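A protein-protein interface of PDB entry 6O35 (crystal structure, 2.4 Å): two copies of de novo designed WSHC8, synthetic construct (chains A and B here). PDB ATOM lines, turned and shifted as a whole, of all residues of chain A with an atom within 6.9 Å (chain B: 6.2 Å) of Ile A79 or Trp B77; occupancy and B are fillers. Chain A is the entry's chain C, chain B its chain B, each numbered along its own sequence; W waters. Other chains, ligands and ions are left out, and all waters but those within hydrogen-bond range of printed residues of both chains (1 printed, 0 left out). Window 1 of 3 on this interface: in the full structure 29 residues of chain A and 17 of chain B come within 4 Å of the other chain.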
ATOM      1  N   GLU A  21       1.051  28.184  21.804  1.00  0.00           N
ATOM      2  CA  GLU A  21       1.686  26.957  22.272  1.00  0.00           C
ATOM      3  C   GLU A  21       0.720  25.783  22.199  1.00  0.00           C
ATOM      4  O   GLU A  21       1.126  24.651  21.905  1.00  0.00           O
ATOM      5  CB  GLU A  21       2.198  27.155  23.700  1.00  0.00           C
ATOM      6  CG  GLU A  21       3.104  26.048  24.212  1.00  0.00           C
ATOM      7  CD  GLU A  21       3.673  26.353  25.587  1.00  0.00           C
ATOM      8  OE1 GLU A  21       4.088  27.508  25.822  1.00  0.00           O
ATOM      9  OE2 GLU A  21       3.698  25.438  26.437  1.00  0.00           O
ATOM     10  N   GLN A  22      -0.567  26.034  22.455  1.00  0.00           N
ATOM     11  CA  GLN A  22      -1.566  24.979  22.324  1.00  0.00           C
ATOM     12  C   GLN A  22      -1.748  24.573  20.867  1.00  0.00           C
ATOM     13  O   GLN A  22      -1.848  23.379  20.559  1.00  0.00           O
ATOM     14  CB  GLN A  22      -2.897  25.438  22.918  1.00  0.00           C
ATOM     15  CG  GLN A  22      -2.919  25.481  24.438  1.00  0.00           C
ATOM     16  N   LYS A  25       0.971  22.115  19.875  1.00  0.00           N
ATOM     17  CA  LYS A  25       0.790  20.748  20.349  1.00  0.00           C
ATOM     18  C   LYS A  25      -0.284  20.021  19.549  1.00  0.00           C
ATOM     19  O   LYS A  25      -0.155  18.822  19.268  1.00  0.00           O
ATOM     20  CB  LYS A  25       0.441  20.756  21.836  1.00  0.00           C
ATOM     21  CG  LYS A  25       1.502  21.411  22.713  1.00  0.00           C
ATOM     22  CD  LYS A  25       2.694  20.489  22.933  1.00  0.00           C
ATOM     23  CE  LYS A  25       2.584  19.760  24.266  1.00  0.00           C
ATOM     24  NZ  LYS A  25       3.433  18.536  24.311  1.00  0.00           N
ATOM     25  N   ALA A  26      -1.350  20.727  19.169  1.00  0.00           N
ATOM     26  CA  ALA A  26      -2.411  20.099  18.390  1.00  0.00           C
ATOM     27  C   ALA A  26      -1.881  19.615  17.046  1.00  0.00           C
ATOM     28  O   ALA A  26      -2.120  18.468  16.647  1.00  0.00           O
ATOM     29  CB  ALA A  26      -3.569  21.076  18.191  1.00  0.00           C
ATOM     30  N   LYS A  27      -1.159  20.480  16.329  1.00  0.00           N
ATOM     31  CA  LYS A  27      -0.572  20.077  15.056  1.00  0.00           C
ATOM     32  C   LYS A  27       0.437  18.953  15.253  1.00  0.00           C
ATOM     33  O   LYS A  27       0.431  17.961  14.516  1.00  0.00           O
ATOM     34  CB  LYS A  27       0.090  21.276  14.377  1.00  0.00           C
ATOM     35  CG  LYS A  27      -0.782  21.964  13.342  1.00  0.00           C
ATOM     36  N   PHE A  29       0.550  16.644  17.386  1.00  0.00           N
ATOM     37  CA  PHE A  29      -0.101  15.359  17.606  1.00  0.00           C
ATOM     38  C   PHE A  29      -0.627  14.783  16.298  1.00  0.00           C
ATOM     39  O   PHE A  29      -0.427  13.598  16.003  1.00  0.00           O
ATOM     40  CB  PHE A  29      -1.238  15.493  18.616  1.00  0.00           C
ATOM     41  CG  PHE A  29      -2.036  14.231  18.780  1.00  0.00           C
ATOM     42  CD1 PHE A  29      -1.579  13.212  19.600  1.00  0.00           C
ATOM     43  CD2 PHE A  29      -3.230  14.055  18.101  1.00  0.00           C
ATOM     44  CE1 PHE A  29      -2.304  12.045  19.748  1.00  0.00           C
ATOM     45  CE2 PHE A  29      -3.957  12.889  18.243  1.00  0.00           C
ATOM     46  CZ  PHE A  29      -3.495  11.885  19.069  1.00  0.00           C
ATOM     47  N   GLN A  30      -1.317  15.607  15.503  1.00  0.00           N
ATOM     48  CA  GLN A  30      -1.849  15.131  14.229  1.00  0.00           C
ATOM     49  C   GLN A  30      -0.739  14.567  13.351  1.00  0.00           C
ATOM     50  O   GLN A  30      -0.917  13.529  12.703  1.00  0.00           O
ATOM     51  CB  GLN A  30      -2.582  16.263  13.511  1.00  0.00           C
ATOM     52  CG  GLN A  30      -3.891  16.668  14.167  1.00  0.00           C
ATOM     53  CD  GLN A  30      -4.925  15.557  14.151  1.00  0.00           C
ATOM     54  OE1 GLN A  30      -5.214  14.976  13.104  1.00  0.00           O
ATOM     55  NE2 GLN A  30      -5.481  15.251  15.316  1.00  0.00           N
ATOM     56  N   ALA A  72      -7.918   7.705  19.395  1.00  0.00           N
ATOM     57  CA  ALA A  72      -6.887   8.726  19.527  1.00  0.00           C
ATOM     58  C   ALA A  72      -7.424  10.100  19.144  1.00  0.00           C
ATOM     59  O   ALA A  72      -7.162  11.092  19.834  1.00  0.00           O
ATOM     60  CB  ALA A  72      -5.678   8.365  18.667  1.00  0.00           C
ATOM     61  N   GLN A  73      -8.172  10.177  18.041  1.00  0.00           N
ATOM     62  CA  GLN A  73      -8.720  11.457  17.607  1.00  0.00           C
ATOM     63  C   GLN A  73      -9.688  12.022  18.641  1.00  0.00           C
ATOM     64  O   GLN A  73      -9.643  13.214  18.959  1.00  0.00           O
ATOM     65  CB  GLN A  73      -9.416  11.296  16.256  1.00  0.00           C
ATOM     66  CG  GLN A  73      -8.471  11.114  15.087  1.00  0.00           C
ATOM     67  CD  GLN A  73      -7.846  12.415  14.628  1.00  0.00           C
ATOM     68  OE1 GLN A  73      -7.916  13.431  15.320  1.00  0.00           O
ATOM     69  NE2 GLN A  73      -7.234  12.393  13.451  1.00  0.00           N
ATOM     70  N   LEU A  74     -10.577  11.179  19.174  1.00  0.00           N
ATOM     71  CA  LEU A  74     -11.525  11.641  20.182  1.00  0.00           C
ATOM     72  C   LEU A  74     -10.808  12.236  21.386  1.00  0.00           C
ATOM     73  O   LEU A  74     -11.217  13.280  21.909  1.00  0.00           O
ATOM     74  CB  LEU A  74     -12.427  10.488  20.615  1.00  0.00           C
ATOM     75  CG  LEU A  74     -13.539  10.120  19.635  1.00  0.00           C
ATOM     76  CD1 LEU A  74     -14.159   8.788  20.019  1.00  0.00           C
ATOM     77  CD2 LEU A  74     -14.597  11.214  19.585  1.00  0.00           C
ATOM     78  N   THR A  75      -9.738  11.584  21.846  1.00  0.00           N
ATOM     79  CA  THR A  75      -8.990  12.100  22.988  1.00  0.00           C
ATOM     80  C   THR A  75      -8.353  13.444  22.655  1.00  0.00           C
ATOM     81  O   THR A  75      -8.437  14.396  23.441  1.00  0.00           O
ATOM     82  CB  THR A  75      -7.925  11.089  23.413  1.00  0.00           C
ATOM     83  OG1 THR A  75      -8.547   9.831  23.704  1.00  0.00           O
ATOM     84  CG2 THR A  75      -7.180  11.581  24.644  1.00  0.00           C
ATOM     85  N   ALA A  76      -7.709  13.540  21.492  1.00  0.00           N
ATOM     86  CA  ALA A  76      -7.129  14.813  21.075  1.00  0.00           C
ATOM     87  C   ALA A  76      -8.211  15.871  20.896  1.00  0.00           C
ATOM     88  O   ALA A  76      -8.024  17.034  21.274  1.00  0.00           O
ATOM     89  CB  ALA A  76      -6.339  14.627  19.779  1.00  0.00           C
ATOM     90  N   TRP A  77      -9.351  15.486  20.317  1.00  0.00           N
ATOM     91  CA  TRP A  77     -10.474  16.409  20.195  1.00  0.00           C
ATOM     92  C   TRP A  77     -10.920  16.906  21.564  1.00  0.00           C
ATOM     93  O   TRP A  77     -11.204  18.097  21.740  1.00  0.00           O
ATOM     94  CB  TRP A  77     -11.627  15.718  19.467  1.00  0.00           C
ATOM     95  CG  TRP A  77     -12.855  16.560  19.303  1.00  0.00           C
ATOM     96  CD1 TRP A  77     -12.934  17.919  19.353  1.00  0.00           C
ATOM     97  CD2 TRP A  77     -14.187  16.090  19.063  1.00  0.00           C
ATOM     98  NE1 TRP A  77     -14.231  18.326  19.159  1.00  0.00           N
ATOM     99  CE2 TRP A  77     -15.021  17.221  18.979  1.00  0.00           C
ATOM    100  CE3 TRP A  77     -14.755  14.821  18.911  1.00  0.00           C
ATOM    101  CZ2 TRP A  77     -16.390  17.123  18.749  1.00  0.00           C
ATOM    102  CZ3 TRP A  77     -16.113  14.726  18.684  1.00  0.00           C
ATOM    103  CH2 TRP A  77     -16.917  15.870  18.605  1.00  0.00           C
ATOM    104  N   GLU A  78     -10.979  16.010  22.549  1.00  0.00           N
ATOM    105  CA  GLU A  78     -11.405  16.403  23.887  1.00  0.00           C
ATOM    106  C   GLU A  78     -10.392  17.332  24.541  1.00  0.00           C
ATOM    107  O   GLU A  78     -10.772  18.268  25.255  1.00  0.00           O
ATOM    108  CB  GLU A  78     -11.637  15.152  24.737  1.00  0.00           C
ATOM    109  CG  GLU A  78     -11.643  15.376  26.242  1.00  0.00           C
ATOM    110  CD  GLU A  78     -12.737  16.319  26.707  1.00  0.00           C
ATOM    111  OE1 GLU A  78     -12.976  16.389  27.932  1.00  0.00           O
ATOM    112  OE2 GLU A  78     -13.358  16.993  25.859  1.00  0.00           O
ATOM    113  N   ILE A  79      -9.099  17.100  24.308  1.00  0.00           N
ATOM    114  CA  ILE A  79      -8.068  17.908  24.953  1.00  0.00           C
ATOM    115  C   ILE A  79      -8.053  19.318  24.372  1.00  0.00           C
ATOM    116  O   ILE A  79      -8.169  20.310  25.101  1.00  0.00           O
ATOM    117  CB  ILE A  79      -6.693  17.233  24.821  1.00  0.00           C
ATOM    118  CG1 ILE A  79      -6.646  15.955  25.659  1.00  0.00           C
ATOM    119  CG2 ILE A  79      -5.591  18.191  25.245  1.00  0.00           C
ATOM    120  CD1 ILE A  79      -5.459  15.066  25.351  1.00  0.00           C
ATOM    121  N   GLU A  80      -7.899  19.428  23.050  1.00  0.00           N
ATOM    122  CA  GLU A  80      -7.826  20.746  22.427  1.00  0.00           C
ATOM    123  C   GLU A  80      -9.114  21.532  22.640  1.00  0.00           C
ATOM    124  O   GLU A  80      -9.078  22.752  22.843  1.00  0.00           O
ATOM    125  CB  GLU A  80      -7.527  20.610  20.935  1.00  0.00           C
ATOM    126  CG  GLU A  80      -6.054  20.740  20.592  1.00  0.00           C
ATOM    127  CD  GLU A  80      -5.478  22.093  20.981  1.00  0.00           C
ATOM    128  OE1 GLU A  80      -6.166  23.119  20.793  1.00  0.00           O
ATOM    129  OE2 GLU A  80      -4.333  22.125  21.481  1.00  0.00           O
ATOM    130  N   SER A  81     -10.263  20.857  22.574  1.00  0.00           N
ATOM    131  CA  SER A  81     -11.528  21.531  22.848  1.00  0.00           C
ATOM    132  C   SER A  81     -11.550  22.086  24.265  1.00  0.00           C
ATOM    133  O   SER A  81     -11.981  23.224  24.490  1.00  0.00           O
ATOM    134  CB  SER A  81     -12.689  20.562  22.635  1.00  0.00           C
ATOM    135  OG  SER A  81     -13.871  21.036  23.255  1.00  0.00           O
ATOM    136  N   LYS A  82     -11.084  21.298  25.234  1.00  0.00           N
ATOM    137  CA  LYS A  82     -11.052  21.764  26.615  1.00  0.00           C
ATOM    138  C   LYS A  82     -10.061  22.909  26.783  1.00  0.00           C
ATOM    139  O   LYS A  82     -10.344  23.884  27.490  1.00  0.00           O
ATOM    140  CB  LYS A  82     -10.696  20.603  27.541  1.00  0.00           C
ATOM    141  CG  LYS A  82     -11.127  20.798  28.980  1.00  0.00           C
ATOM    142  CD  LYS A  82     -10.251  19.993  29.928  1.00  0.00           C
ATOM    143  N   SER A  83      -8.896  22.814  26.136  1.00  0.00           N
ATOM    144  CA  SER A  83      -7.891  23.865  26.252  1.00  0.00           C
ATOM    145  C   SER A  83      -8.382  25.167  25.634  1.00  0.00           C
ATOM    146  O   SER A  83      -8.343  26.224  26.275  1.00  0.00           O
ATOM    147  CB  SER A  83      -6.588  23.422  25.585  1.00  0.00           C
ATOM    148  OG  SER A  83      -5.939  22.416  26.340  1.00  0.00           O
ATOM    149  N   LYS A  84      -8.847  25.114  24.383  1.00  0.00           N
ATOM    150  CA  LYS A  84      -9.282  26.328  23.702  1.00  0.00           C
ATOM    151  C   LYS A  84     -10.361  27.050  24.498  1.00  0.00           C
ATOM    152  O   LYS A  84     -10.346  28.282  24.602  1.00  0.00           O
ATOM    153  CB  LYS A  84      -9.790  25.985  22.302  1.00  0.00           C
ATOM    154  CG  LYS A  84     -10.267  27.185  21.505  1.00  0.00           C
ATOM    155  N   ILE A  85     -11.307  26.301  25.068  1.00  0.00           N
ATOM    156  CA  ILE A  85     -12.392  26.923  25.818  1.00  0.00           C
ATOM    157  C   ILE A  85     -11.867  27.553  27.101  1.00  0.00           C
ATOM    158  O   ILE A  85     -12.281  28.653  27.482  1.00  0.00           O
ATOM    159  CB  ILE A  85     -13.496  25.889  26.103  1.00  0.00           C
ATOM    160  CG1 ILE A  85     -14.349  25.670  24.853  1.00  0.00           C
ATOM    161  CG2 ILE A  85     -14.363  26.343  27.264  1.00  0.00           C
ATOM    162  CD1 ILE A  85     -15.094  24.353  24.844  1.00  0.00           C
ATOM    163  N   ALA B  72       0.292   7.531  26.003  1.00  0.00           N
ATOM    164  CA  ALA B  72       1.121   8.229  26.978  1.00  0.00           C
ATOM    165  C   ALA B  72       1.258   9.705  26.623  1.00  0.00           C
ATOM    166  O   ALA B  72       1.098  10.580  27.481  1.00  0.00           O
ATOM    167  CB  ALA B  72       2.495   7.564  27.065  1.00  0.00           C
ATOM    168  N   GLN B  73       1.559  10.002  25.356  1.00  0.00           N
ATOM    169  CA  GLN B  73       1.700  11.391  24.934  1.00  0.00           C
ATOM    170  C   GLN B  73       0.412  12.172  25.166  1.00  0.00           C
ATOM    171  O   GLN B  73       0.444  13.312  25.641  1.00  0.00           O
ATOM    172  CB  GLN B  73       2.103  11.457  23.461  1.00  0.00           C
ATOM    173  CG  GLN B  73       3.576  11.203  23.202  1.00  0.00           C
ATOM    174  CD  GLN B  73       4.459  12.351  23.653  1.00  0.00           C
ATOM    175  OE1 GLN B  73       4.004  13.282  24.318  1.00  0.00           O
ATOM    176  NE2 GLN B  73       5.734  12.291  23.287  1.00  0.00           N
ATOM    177  N   LEU B  74      -0.736  11.577  24.827  1.00  0.00           N
ATOM    178  CA  LEU B  74      -2.012  12.250  25.048  1.00  0.00           C
ATOM    179  C   LEU B  74      -2.233  12.546  26.526  1.00  0.00           C
ATOM    180  O   LEU B  74      -2.741  13.617  26.885  1.00  0.00           O
ATOM    181  CB  LEU B  74      -3.154  11.392  24.503  1.00  0.00           C
ATOM    182  CG  LEU B  74      -3.334  11.392  22.986  1.00  0.00           C
ATOM    183  CD1 LEU B  74      -4.168  10.201  22.540  1.00  0.00           C
ATOM    184  CD2 LEU B  74      -3.975  12.696  22.529  1.00  0.00           C
ATOM    185  N   THR B  75      -1.864  11.609  27.400  1.00  0.00           N
ATOM    186  CA  THR B  75      -2.057  11.813  28.832  1.00  0.00           C
ATOM    187  C   THR B  75      -1.164  12.934  29.352  1.00  0.00           C
ATOM    188  O   THR B  75      -1.630  13.839  30.054  1.00  0.00           O
ATOM    189  CB  THR B  75      -1.788  10.509  29.584  1.00  0.00           C
ATOM    190  OG1 THR B  75      -2.678   9.489  29.113  1.00  0.00           O
ATOM    191  CG2 THR B  75      -1.986  10.701  31.078  1.00  0.00           C
ATOM    192  N   ALA B  76       0.127  12.892  29.020  1.00  0.00           N
ATOM    193  CA  ALA B  76       1.023  13.969  29.426  1.00  0.00           C
ATOM    194  C   ALA B  76       0.583  15.298  28.823  1.00  0.00           C
ATOM    195  O   ALA B  76       0.720  16.354  29.454  1.00  0.00           O
ATOM    196  CB  ALA B  76       2.458  13.640  29.015  1.00  0.00           C
ATOM    197  N   TRP B  77       0.055  15.265  27.598  1.00  0.00           N
ATOM    198  CA  TRP B  77      -0.492  16.472  26.987  1.00  0.00           C
ATOM    199  C   TRP B  77      -1.701  16.975  27.765  1.00  0.00           C
ATOM    200  O   TRP B  77      -1.888  18.188  27.924  1.00  0.00           O
ATOM    201  CB  TRP B  77      -0.860  16.182  25.533  1.00  0.00           C
ATOM    202  CG  TRP B  77      -1.484  17.324  24.800  1.00  0.00           C
ATOM    203  CD1 TRP B  77      -1.395  18.651  25.106  1.00  0.00           C
ATOM    204  CD2 TRP B  77      -2.302  17.237  23.627  1.00  0.00           C
ATOM    205  NE1 TRP B  77      -2.107  19.395  24.196  1.00  0.00           N
ATOM    206  CE2 TRP B  77      -2.673  18.550  23.279  1.00  0.00           C
ATOM    207  CE3 TRP B  77      -2.754  16.176  22.838  1.00  0.00           C
ATOM    208  CZ2 TRP B  77      -3.474  18.830  22.177  1.00  0.00           C
ATOM    209  CZ3 TRP B  77      -3.550  16.455  21.745  1.00  0.00           C
ATOM    210  CH2 TRP B  77      -3.904  17.771  21.424  1.00  0.00           C
ATOM    211  N   GLU B  78      -2.531  16.059  28.265  1.00  0.00           N
ATOM    212  CA  GLU B  78      -3.691  16.463  29.050  1.00  0.00           C
ATOM    213  C   GLU B  78      -3.268  17.062  30.384  1.00  0.00           C
ATOM    214  O   GLU B  78      -3.845  18.059  30.836  1.00  0.00           O
ATOM    215  CB  GLU B  78      -4.613  15.264  29.265  1.00  0.00           C
ATOM    216  CG  GLU B  78      -5.947  15.607  29.897  1.00  0.00           C
ATOM    217  N   ILE B  79      -2.255  16.476  31.024  1.00  0.00           N
ATOM    218  CA  ILE B  79      -1.809  16.965  32.325  1.00  0.00           C
ATOM    219  C   ILE B  79      -1.201  18.356  32.192  1.00  0.00           C
ATOM    220  O   ILE B  79      -1.591  19.290  32.903  1.00  0.00           O
ATOM    221  CB  ILE B  79      -0.809  15.974  32.952  1.00  0.00           C
ATOM    222  CG1 ILE B  79      -1.527  14.686  33.363  1.00  0.00           C
ATOM    223  CG2 ILE B  79      -0.101  16.614  34.135  1.00  0.00           C
ATOM    224  CD1 ILE B  79      -0.591  13.545  33.700  1.00  0.00           C
ATOM    225  N   GLU B  80      -0.229  18.513  31.289  1.00  0.00           N
ATOM    226  CA  GLU B  80       0.456  19.794  31.156  1.00  0.00           C
ATOM    227  C   GLU B  80      -0.486  20.878  30.647  1.00  0.00           C
ATOM    228  O   GLU B  80      -0.410  22.030  31.089  1.00  0.00           O
ATOM    229  CB  GLU B  80       1.657  19.655  30.224  1.00  0.00           C
ATOM    230  CG  GLU B  80       2.950  19.319  30.943  1.00  0.00           C
ATOM    231  CD  GLU B  80       3.326  20.363  31.981  1.00  0.00           C
ATOM    232  OE1 GLU B  80       2.962  21.546  31.801  1.00  0.00           O
ATOM    233  OE2 GLU B  80       3.975  19.996  32.983  1.00  0.00           O
ATOM    234  N   SER B  81      -1.369  20.537  29.707  1.00  0.00           N
ATOM    235  CA  SER B  81      -2.345  21.509  29.228  1.00  0.00           C
ATOM    236  C   SER B  81      -3.246  21.980  30.362  1.00  0.00           C
ATOM    237  O   SER B  81      -3.563  23.171  30.461  1.00  0.00           O
ATOM    238  CB  SER B  81      -3.174  20.901  28.097  1.00  0.00           C
ATOM    239  OG  SER B  81      -4.279  21.723  27.768  1.00  0.00           O
ATOM    240  N   LYS B  82      -3.662  21.060  31.236  1.00  0.00           N
ATOM    241  CA  LYS B  82      -4.482  21.445  32.378  1.00  0.00           C
ATOM    242  C   LYS B  82      -3.683  22.272  33.378  1.00  0.00           C
ATOM    243  O   LYS B  82      -4.186  23.271  33.906  1.00  0.00           O
ATOM    244  CB  LYS B  82      -5.055  20.200  33.056  1.00  0.00           C
ATOM    245  CG  LYS B  82      -6.461  19.845  32.605  1.00  0.00           C
HETATM  246  O   HOH W   1      -3.758  22.226  24.916  1.00  0.00           O
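OG of Ser A83 sits close to OG of Ser B81 (2.3 Å).
The side-chain hydroxyl of Ser A83 lies within hydrogen-bond range of the backbone carbonyl oxygen of Ile A79 (3.3 Å).
Lys A25 touches Trp B77 (CB to NE1, 3.7 Å). Leu B74 touches Phe A29 (CD2 to CE1, 3.3 Å). Leu B74 touches Thr A75 (CD1 to CG2, 3.9 Å). N of Ala A76 touches CD2 of Leu B74, 3.97 Å away. Ala A76 touches Trp B77 (CB to CZ3, 3.9 Å). Leu B74 touches Ile A79. Ile A79 touches Trp B77. Glu A80 touches Trp B77 (OE2 to CZ2, 3.5 Å).
Of the printed residues of chain B, Ile A79 touches Leu B74 and Trp B77. Printed residues of chain A within 4 Å of Trp B77: Lys A25 (3.7 Å), Ala A76 (3.9 Å), Ile A79 (3.5 Å) and Glu A80 (3.5 Å). Printed residues of chain A within 4 Å of Ser B81: Ser A83. Printed residues of chain B within 4 Å of Lys A25: Trp B77 (3.7 Å). Printed residues of chain B within 4 Å of Glu A80: Trp B77 (3.5 Å). Lys B82 touches none of the printed residues of chain A. Glu A78 touches none of the printed residues of chain B. The nearest printed residue of chain B that does not touch Ile A79 is Glu B78 (4.01 Å). The nearest printed residue of chain B that does not touch Glu A80 is Ser B81 (6.3 Å).
Printed residues of chain A that touch a printed residue of chain B: Lys A25, Phe A29, Thr A75, Ala A76, Ile A79, Glu A80 and Ser A83. Printed residues of chain B that touch a printed residue of chain A: Leu B74, Trp B77 and Ser B81. Hydrophobic or aromatic side chains of chain B within 4 Å of the printed part of chain A: Leu B74 and Trp B77.
Thr A75 touches Leu B74, but with the chains exchanged Leu A74 does not touch Thr B75 (10.8 Å). Ala A76 touches Leu B74, but with the chains exchanged Leu A74 does not touch Ala B76 (13.4 Å). Ile A79 touches Leu B74, but with the chains exchanged Leu A74 does not touch Ile B79 (13.2 Å). Glu A80 touches Trp B77, but with the chains exchanged Trp A77 does not touch Glu B80 (14.2 Å).
Water W1 lies within hydrogen-bond range of OG of Ser A83, OG of Ser B81, NE1 of Trp B77 and OE2 of Glu A80.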
